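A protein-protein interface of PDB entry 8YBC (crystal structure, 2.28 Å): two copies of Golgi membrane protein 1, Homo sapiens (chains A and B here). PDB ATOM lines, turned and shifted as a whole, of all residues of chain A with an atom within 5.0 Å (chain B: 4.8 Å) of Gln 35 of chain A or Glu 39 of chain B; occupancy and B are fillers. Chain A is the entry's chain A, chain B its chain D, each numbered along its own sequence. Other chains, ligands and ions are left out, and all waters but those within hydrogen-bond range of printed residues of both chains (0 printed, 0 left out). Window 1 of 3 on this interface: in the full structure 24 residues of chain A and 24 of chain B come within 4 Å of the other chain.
NE2 of Gln 35 of chain A lies within hydrogen-bond range of OE2 of Glu 39 of chain B (2.6 Å).
Among the printed residues, pairs that only touch across the chains: Leu 38 of chain A with Glu 39 of chain B, Phe 42 of chain A with Glu 39 of chain B, Phe 42 of chain A with Ser 43 of chain B and Phe 42 of chain A with Phe 42 of chain B.
Of chain B, only Glu 39 comes within 4 Å of Gln 35 of chain A. Of the printed residues of chain A, Phe 42 of chain B touches Phe 42 (3.8 Å). Printed residues of chain A within 4 Å of Ser 43 of chain B: Phe 42. Asn 37 of chain A touches none of the printed residues of chain B. Thr 36 of chain B touches none of the printed residues of chain A. The nearest residue of chain B that does not touch Gln 35 of chain A is Gln 35 of chain B (4.3 Å). The nearest printed residue of chain A that does not touch Glu 39 of chain B is Glu 39 of chain A (5.5 Å). The nearest printed residue of chain A that does not touch Ser 43 of chain B is Leu 38 of chain A (7.0 Å).
Of the 10 printed residues of chain B, 3 touch a printed residue of chain A. Printed residues of chain A that touch a printed residue of chain B: Gln 35, Leu 38 and Phe 42. Among the printed residues, 5 pairs touch across the chains. Among the printed residues, no Asp or Glu carboxylate lies within 4 Å of a Lys or Arg side-chain nitrogen of the other chain.
Gln 35 of chain A touches Glu 39 of chain B, but with the chains exchanged Glu 39 of chain A does not touch Gln 35 of chain B (6.1 Å). Leu 38 of chain A touches Glu 39 of chain B, but with the chains exchanged Glu 39 of chain A does not touch Leu 38 of chain B (11.2 Å). Phe 42 of chain A touches Glu 39 of chain B, but with the chains exchanged Glu 39 of chain A does not touch Phe 42 of chain B (7.0 Å). Phe 42 of chain B touches its own counterpart, Phe 42 of chain A. Positions printed for both chains: 35, 36, 37, 38, 39 and 42.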
ATOM      1  N   PHE A  31     -19.802  28.185  20.773  1.00  0.00           N
ATOM      2  CA  PHE A  31     -19.407  27.677  22.084  1.00  0.00           C
ATOM      3  C   PHE A  31     -20.535  26.895  22.742  1.00  0.00           C
ATOM      4  O   PHE A  31     -20.376  25.711  23.071  1.00  0.00           O
ATOM      5  CB  PHE A  31     -18.952  28.834  22.984  1.00  0.00           C
ATOM      6  CG  PHE A  31     -18.772  28.450  24.432  1.00  0.00           C
ATOM      7  CD1 PHE A  31     -17.587  27.871  24.866  1.00  0.00           C
ATOM      8  CD2 PHE A  31     -19.783  28.680  25.359  1.00  0.00           C
ATOM      9  CE1 PHE A  31     -17.409  27.519  26.195  1.00  0.00           C
ATOM     10  CE2 PHE A  31     -19.615  28.332  26.689  1.00  0.00           C
ATOM     11  CZ  PHE A  31     -18.421  27.747  27.103  1.00  0.00           C
ATOM     12  N   GLN A  32     -21.693  27.538  22.924  1.00  0.00           N
ATOM     13  CA  GLN A  32     -22.760  26.939  23.729  1.00  0.00           C
ATOM     14  C   GLN A  32     -23.265  25.629  23.129  1.00  0.00           C
ATOM     15  O   GLN A  32     -23.530  24.665  23.860  1.00  0.00           O
ATOM     16  CB  GLN A  32     -23.915  27.924  23.888  1.00  0.00           C
ATOM     17  CG  GLN A  32     -23.534  29.188  24.653  1.00  0.00           C
ATOM     18  CD  GLN A  32     -24.715  30.113  24.894  1.00  0.00           C
ATOM     19  OE1 GLN A  32     -25.713  30.074  24.170  1.00  0.00           O
ATOM     20  NE2 GLN A  32     -24.610  30.949  25.925  1.00  0.00           N
ATOM     21  N   LYS A  33     -23.417  25.569  21.807  1.00  0.00           N
ATOM     22  CA  LYS A  33     -23.895  24.322  21.210  1.00  0.00           C
ATOM     23  C   LYS A  33     -22.863  23.213  21.371  1.00  0.00           C
ATOM     24  O   LYS A  33     -23.217  22.066  21.670  1.00  0.00           O
ATOM     25  CB  LYS A  33     -24.255  24.537  19.743  1.00  0.00           C
ATOM     26  CG  LYS A  33     -25.512  25.374  19.547  1.00  0.00           C
ATOM     27  CD  LYS A  33     -26.663  24.896  20.426  1.00  0.00           C
ATOM     28  CE  LYS A  33     -27.801  25.920  20.448  1.00  0.00           C
ATOM     29  NZ  LYS A  33     -28.250  26.268  19.069  1.00  0.00           N
ATOM     30  N   ASN A  34     -21.581  23.545  21.216  1.00  0.00           N
ATOM     31  CA  ASN A  34     -20.510  22.592  21.491  1.00  0.00           C
ATOM     32  C   ASN A  34     -20.430  22.198  22.961  1.00  0.00           C
ATOM     33  O   ASN A  34     -19.783  21.203  23.287  1.00  0.00           O
ATOM     34  CB  ASN A  34     -19.158  23.163  21.053  1.00  0.00           C
ATOM     35  CG  ASN A  34     -18.030  22.169  21.218  1.00  0.00           C
ATOM     36  OD1 ASN A  34     -17.809  21.320  20.350  1.00  0.00           O
ATOM     37  ND2 ASN A  34     -17.327  22.243  22.357  1.00  0.00           N
ATOM     38  N   GLN A  35     -21.060  22.942  23.865  1.00  0.00           N
ATOM     39  CA  GLN A  35     -20.933  22.576  25.269  1.00  0.00           C
ATOM     40  C   GLN A  35     -21.714  21.310  25.596  1.00  0.00           C
ATOM     41  O   GLN A  35     -21.368  20.601  26.547  1.00  0.00           O
ATOM     42  CB  GLN A  35     -21.395  23.731  26.153  1.00  0.00           C
ATOM     43  CG  GLN A  35     -20.294  24.746  26.405  1.00  0.00           C
ATOM     44  CD  GLN A  35     -19.113  24.121  27.120  1.00  0.00           C
ATOM     45  OE1 GLN A  35     -17.966  24.290  26.714  1.00  0.00           O
ATOM     46  NE2 GLN A  35     -19.395  23.373  28.181  1.00  0.00           N
ATOM     47  N   THR A  36     -22.750  21.008  24.810  1.00  0.00           N
ATOM     48  CA  THR A  36     -23.672  19.922  25.133  1.00  0.00           C
ATOM     49  C   THR A  36     -22.981  18.569  25.107  1.00  0.00           C
ATOM     50  O   THR A  36     -23.205  17.735  25.993  1.00  0.00           O
ATOM     51  CB  THR A  36     -24.833  19.935  24.141  1.00  0.00           C
ATOM     52  OG1 THR A  36     -25.520  21.192  24.232  1.00  0.00           O
ATOM     53  CG2 THR A  36     -25.796  18.756  24.392  1.00  0.00           C
ATOM     54  N   ASN A  37     -22.150  18.321  24.091  1.00  0.00           N
ATOM     55  CA  ASN A  37     -21.504  17.019  24.009  1.00  0.00           C
ATOM     56  C   ASN A  37     -20.504  16.839  25.141  1.00  0.00           C
ATOM     57  O   ASN A  37     -20.318  15.719  25.625  1.00  0.00           O
ATOM     58  CB  ASN A  37     -20.848  16.814  22.634  1.00  0.00           C
ATOM     59  CG  ASN A  37     -19.620  17.689  22.409  1.00  0.00           C
ATOM     60  OD1 ASN A  37     -19.735  18.849  22.042  1.00  0.00           O
ATOM     61  ND2 ASN A  37     -18.442  17.114  22.574  1.00  0.00           N
ATOM     62  N   LEU A  38     -19.905  17.938  25.615  1.00  0.00           N
ATOM     63  CA  LEU A  38     -18.982  17.859  26.737  1.00  0.00           C
ATOM     64  C   LEU A  38     -19.724  17.615  28.047  1.00  0.00           C
ATOM     65  O   LEU A  38     -19.271  16.814  28.869  1.00  0.00           O
ATOM     66  CB  LEU A  38     -18.133  19.138  26.824  1.00  0.00           C
ATOM     67  CG  LEU A  38     -17.161  19.365  25.664  1.00  0.00           C
ATOM     68  CD1 LEU A  38     -16.454  20.727  25.767  1.00  0.00           C
ATOM     69  CD2 LEU A  38     -16.144  18.243  25.586  1.00  0.00           C
ATOM     70  N   GLU A  39     -20.841  18.316  28.276  1.00  0.00           N
ATOM     71  CA  GLU A  39     -21.599  18.082  29.502  1.00  0.00           C
ATOM     72  C   GLU A  39     -22.059  16.628  29.581  1.00  0.00           C
ATOM     73  O   GLU A  39     -21.967  15.989  30.639  1.00  0.00           O
ATOM     74  CB  GLU A  39     -22.790  19.031  29.584  1.00  0.00           C
ATOM     75  CG  GLU A  39     -22.395  20.500  29.788  1.00  0.00           C
ATOM     76  CD  GLU A  39     -23.585  21.469  29.736  1.00  0.00           C
ATOM     77  OE1 GLU A  39     -23.595  22.455  30.518  1.00  0.00           O
ATOM     78  OE2 GLU A  39     -24.509  21.245  28.914  1.00  0.00           O
ATOM     79  N   PHE A  42     -19.051  14.402  30.594  1.00  0.00           N
ATOM     80  CA  PHE A  42     -18.725  14.408  32.024  1.00  0.00           C
ATOM     81  C   PHE A  42     -19.739  13.608  32.824  1.00  0.00           C
ATOM     82  O   PHE A  42     -19.370  12.833  33.707  1.00  0.00           O
ATOM     83  CB  PHE A  42     -18.690  15.821  32.589  1.00  0.00           C
ATOM     84  CG  PHE A  42     -17.797  16.722  31.871  1.00  0.00           C
ATOM     85  CD1 PHE A  42     -16.629  16.259  31.325  1.00  0.00           C
ATOM     86  CD2 PHE A  42     -18.161  18.044  31.693  1.00  0.00           C
ATOM     87  CE1 PHE A  42     -15.805  17.129  30.620  1.00  0.00           C
ATOM     88  CE2 PHE A  42     -17.368  18.899  30.990  1.00  0.00           C
ATOM     89  CZ  PHE A  42     -16.184  18.453  30.455  1.00  0.00           C
ATOM     90  N   GLN B  35     -13.638  28.362  31.124  1.00  0.00           N
ATOM     91  CA  GLN B  35     -14.445  27.162  31.266  1.00  0.00           C
ATOM     92  C   GLN B  35     -13.840  26.014  30.479  1.00  0.00           C
ATOM     93  O   GLN B  35     -13.848  24.877  30.952  1.00  0.00           O
ATOM     94  CB  GLN B  35     -15.897  27.412  30.875  1.00  0.00           C
ATOM     95  CG  GLN B  35     -16.780  26.302  31.406  1.00  0.00           C
ATOM     96  CD  GLN B  35     -18.101  26.794  31.886  1.00  0.00           C
ATOM     97  OE1 GLN B  35     -18.189  27.333  32.984  1.00  0.00           O
ATOM     98  NE2 GLN B  35     -19.153  26.603  31.081  1.00  0.00           N
ATOM     99  N   THR B  36     -13.218  26.306  29.335  1.00  0.00           N
ATOM    100  CA  THR B  36     -12.557  25.244  28.579  1.00  0.00           C
ATOM    101  C   THR B  36     -11.306  24.716  29.299  1.00  0.00           C
ATOM    102  O   THR B  36     -11.017  23.512  29.244  1.00  0.00           O
ATOM    103  CB  THR B  36     -12.211  25.751  27.173  1.00  0.00           C
ATOM    104  OG1 THR B  36     -12.146  24.649  26.263  1.00  0.00           O
ATOM    105  CG2 THR B  36     -10.859  26.451  27.152  1.00  0.00           C
ATOM    106  N   ASN B  37     -10.565  25.591  29.989  1.00  0.00           N
ATOM    107  CA  ASN B  37      -9.384  25.141  30.715  1.00  0.00           C
ATOM    108  C   ASN B  37      -9.781  24.321  31.943  1.00  0.00           C
ATOM    109  O   ASN B  37      -9.199  23.278  32.220  1.00  0.00           O
ATOM    110  CB  ASN B  37      -8.525  26.355  31.103  1.00  0.00           C
ATOM    111  CG  ASN B  37      -7.788  26.972  29.897  1.00  0.00           C
ATOM    112  OD1 ASN B  37      -7.372  26.263  28.981  1.00  0.00           O
ATOM    113  ND2 ASN B  37      -7.651  28.298  29.893  1.00  0.00           N
ATOM    114  N   LEU B  38     -10.805  24.759  32.660  1.00  0.00           N
ATOM    115  CA  LEU B  38     -11.294  24.006  33.802  1.00  0.00           C
ATOM    116  C   LEU B  38     -11.888  22.654  33.402  1.00  0.00           C
ATOM    117  O   LEU B  38     -11.851  21.702  34.195  1.00  0.00           O
ATOM    118  CB  LEU B  38     -12.329  24.850  34.525  1.00  0.00           C
ATOM    119  CG  LEU B  38     -12.864  24.347  35.848  1.00  0.00           C
ATOM    120  CD1 LEU B  38     -11.716  23.992  36.845  1.00  0.00           C
ATOM    121  CD2 LEU B  38     -13.768  25.449  36.367  1.00  0.00           C
ATOM    122  N   GLU B  39     -12.444  22.553  32.187  1.00  0.00           N
ATOM    123  CA  GLU B  39     -13.031  21.299  31.712  1.00  0.00           C
ATOM    124  C   GLU B  39     -11.957  20.272  31.382  1.00  0.00           C
ATOM    125  O   GLU B  39     -12.150  19.069  31.603  1.00  0.00           O
ATOM    126  CB  GLU B  39     -13.892  21.554  30.472  1.00  0.00           C
ATOM    127  CG  GLU B  39     -15.325  21.903  30.768  1.00  0.00           C
ATOM    128  CD  GLU B  39     -16.079  22.344  29.507  1.00  0.00           C
ATOM    129  OE1 GLU B  39     -15.434  22.474  28.448  1.00  0.00           O
ATOM    130  OE2 GLU B  39     -17.309  22.553  29.576  1.00  0.00           O
ATOM    131  N   ARG B  40     -10.845  20.725  30.806  1.00  0.00           N
ATOM    132  CA  ARG B  40      -9.686  19.861  30.619  1.00  0.00           C
ATOM    133  C   ARG B  40      -9.263  19.231  31.941  1.00  0.00           C
ATOM    134  O   ARG B  40      -8.978  18.034  32.004  1.00  0.00           O
ATOM    135  CB  ARG B  40      -8.532  20.662  30.012  1.00  0.00           C
ATOM    136  CG  ARG B  40      -8.785  21.126  28.592  1.00  0.00           C
ATOM    137  CD  ARG B  40      -7.475  21.386  27.849  1.00  0.00           C
ATOM    138  NE  ARG B  40      -7.405  22.730  27.279  1.00  0.00           N
ATOM    139  CZ  ARG B  40      -6.457  23.620  27.572  1.00  0.00           C
ATOM    140  NH1 ARG B  40      -5.495  23.311  28.431  1.00  0.00           N
ATOM    141  NH2 ARG B  40      -6.457  24.818  27.000  1.00  0.00           N
ATOM    142  N   LYS B  41      -9.245  20.030  33.009  1.00  0.00           N
ATOM    143  CA  LYS B  41      -8.896  19.525  34.334  1.00  0.00           C
ATOM    144  C   LYS B  41      -9.986  18.613  34.879  1.00  0.00           C
ATOM    145  O   LYS B  41      -9.696  17.554  35.428  1.00  0.00           O
ATOM    146  CB  LYS B  41      -8.643  20.694  35.298  1.00  0.00           C
ATOM    147  CG  LYS B  41      -7.915  20.250  36.575  1.00  0.00           C
ATOM    148  CD  LYS B  41      -7.837  21.348  37.623  1.00  0.00           C
ATOM    149  CE  LYS B  41      -7.095  20.840  38.866  1.00  0.00           C
ATOM    150  NZ  LYS B  41      -7.820  19.745  39.565  1.00  0.00           N
ATOM    151  N   PHE B  42     -11.243  19.025  34.752  1.00  0.00           N
ATOM    152  CA  PHE B  42     -12.371  18.231  35.231  1.00  0.00           C
ATOM    153  C   PHE B  42     -12.413  16.860  34.557  1.00  0.00           C
ATOM    154  O   PHE B  42     -12.681  15.845  35.210  1.00  0.00           O
ATOM    155  CB  PHE B  42     -13.662  19.006  34.969  1.00  0.00           C
ATOM    156  CG  PHE B  42     -14.890  18.440  35.624  1.00  0.00           C
ATOM    157  CD1 PHE B  42     -14.919  18.162  36.984  1.00  0.00           C
ATOM    158  CD2 PHE B  42     -16.054  18.255  34.878  1.00  0.00           C
ATOM    159  CE1 PHE B  42     -16.062  17.683  37.572  1.00  0.00           C
ATOM    160  CE2 PHE B  42     -17.203  17.778  35.465  1.00  0.00           C
ATOM    161  CZ  PHE B  42     -17.208  17.478  36.810  1.00  0.00           C
ATOM    162  N   SER B  43     -12.124  16.816  33.254  1.00  0.00           N
ATOM    163  CA  SER B  43     -12.174  15.569  32.505  1.00  0.00           C
ATOM    164  C   SER B  43     -10.946  14.715  32.807  1.00  0.00           C
ATOM    165  O   SER B  43     -11.027  13.479  32.836  1.00  0.00           O
ATOM    166  CB  SER B  43     -12.322  15.884  31.007  1.00  0.00           C
ATOM    167  OG  SER B  43     -11.743  14.900  30.176  1.00  0.00           O
ATOM    168  N   TYR B  44      -9.817  15.353  33.095  1.00  0.00           N
ATOM    169  CA  TYR B  44      -8.674  14.604  33.618  1.00  0.00           C
ATOM    170  C   TYR B  44      -9.012  13.919  34.948  1.00  0.00           C
ATOM    171  O   TYR B  44      -8.773  12.720  35.121  1.00  0.00           O
ATOM    172  CB  TYR B  44      -7.471  15.532  33.758  1.00  0.00           C
ATOM    173  CG  TYR B  44      -6.209  14.767  34.002  1.00  0.00           C
ATOM    174  CD1 TYR B  44      -5.670  13.962  33.005  1.00  0.00           C
ATOM    175  CD2 TYR B  44      -5.581  14.797  35.249  1.00  0.00           C
ATOM    176  CE1 TYR B  44      -4.517  13.223  33.229  1.00  0.00           C
ATOM    177  CE2 TYR B  44      -4.424  14.067  35.485  1.00  0.00           C
ATOM    178  CZ  TYR B  44      -3.899  13.282  34.470  1.00  0.00           C
ATOM    179  OH  TYR B  44      -2.774  12.540  34.681  1.00  0.00           O
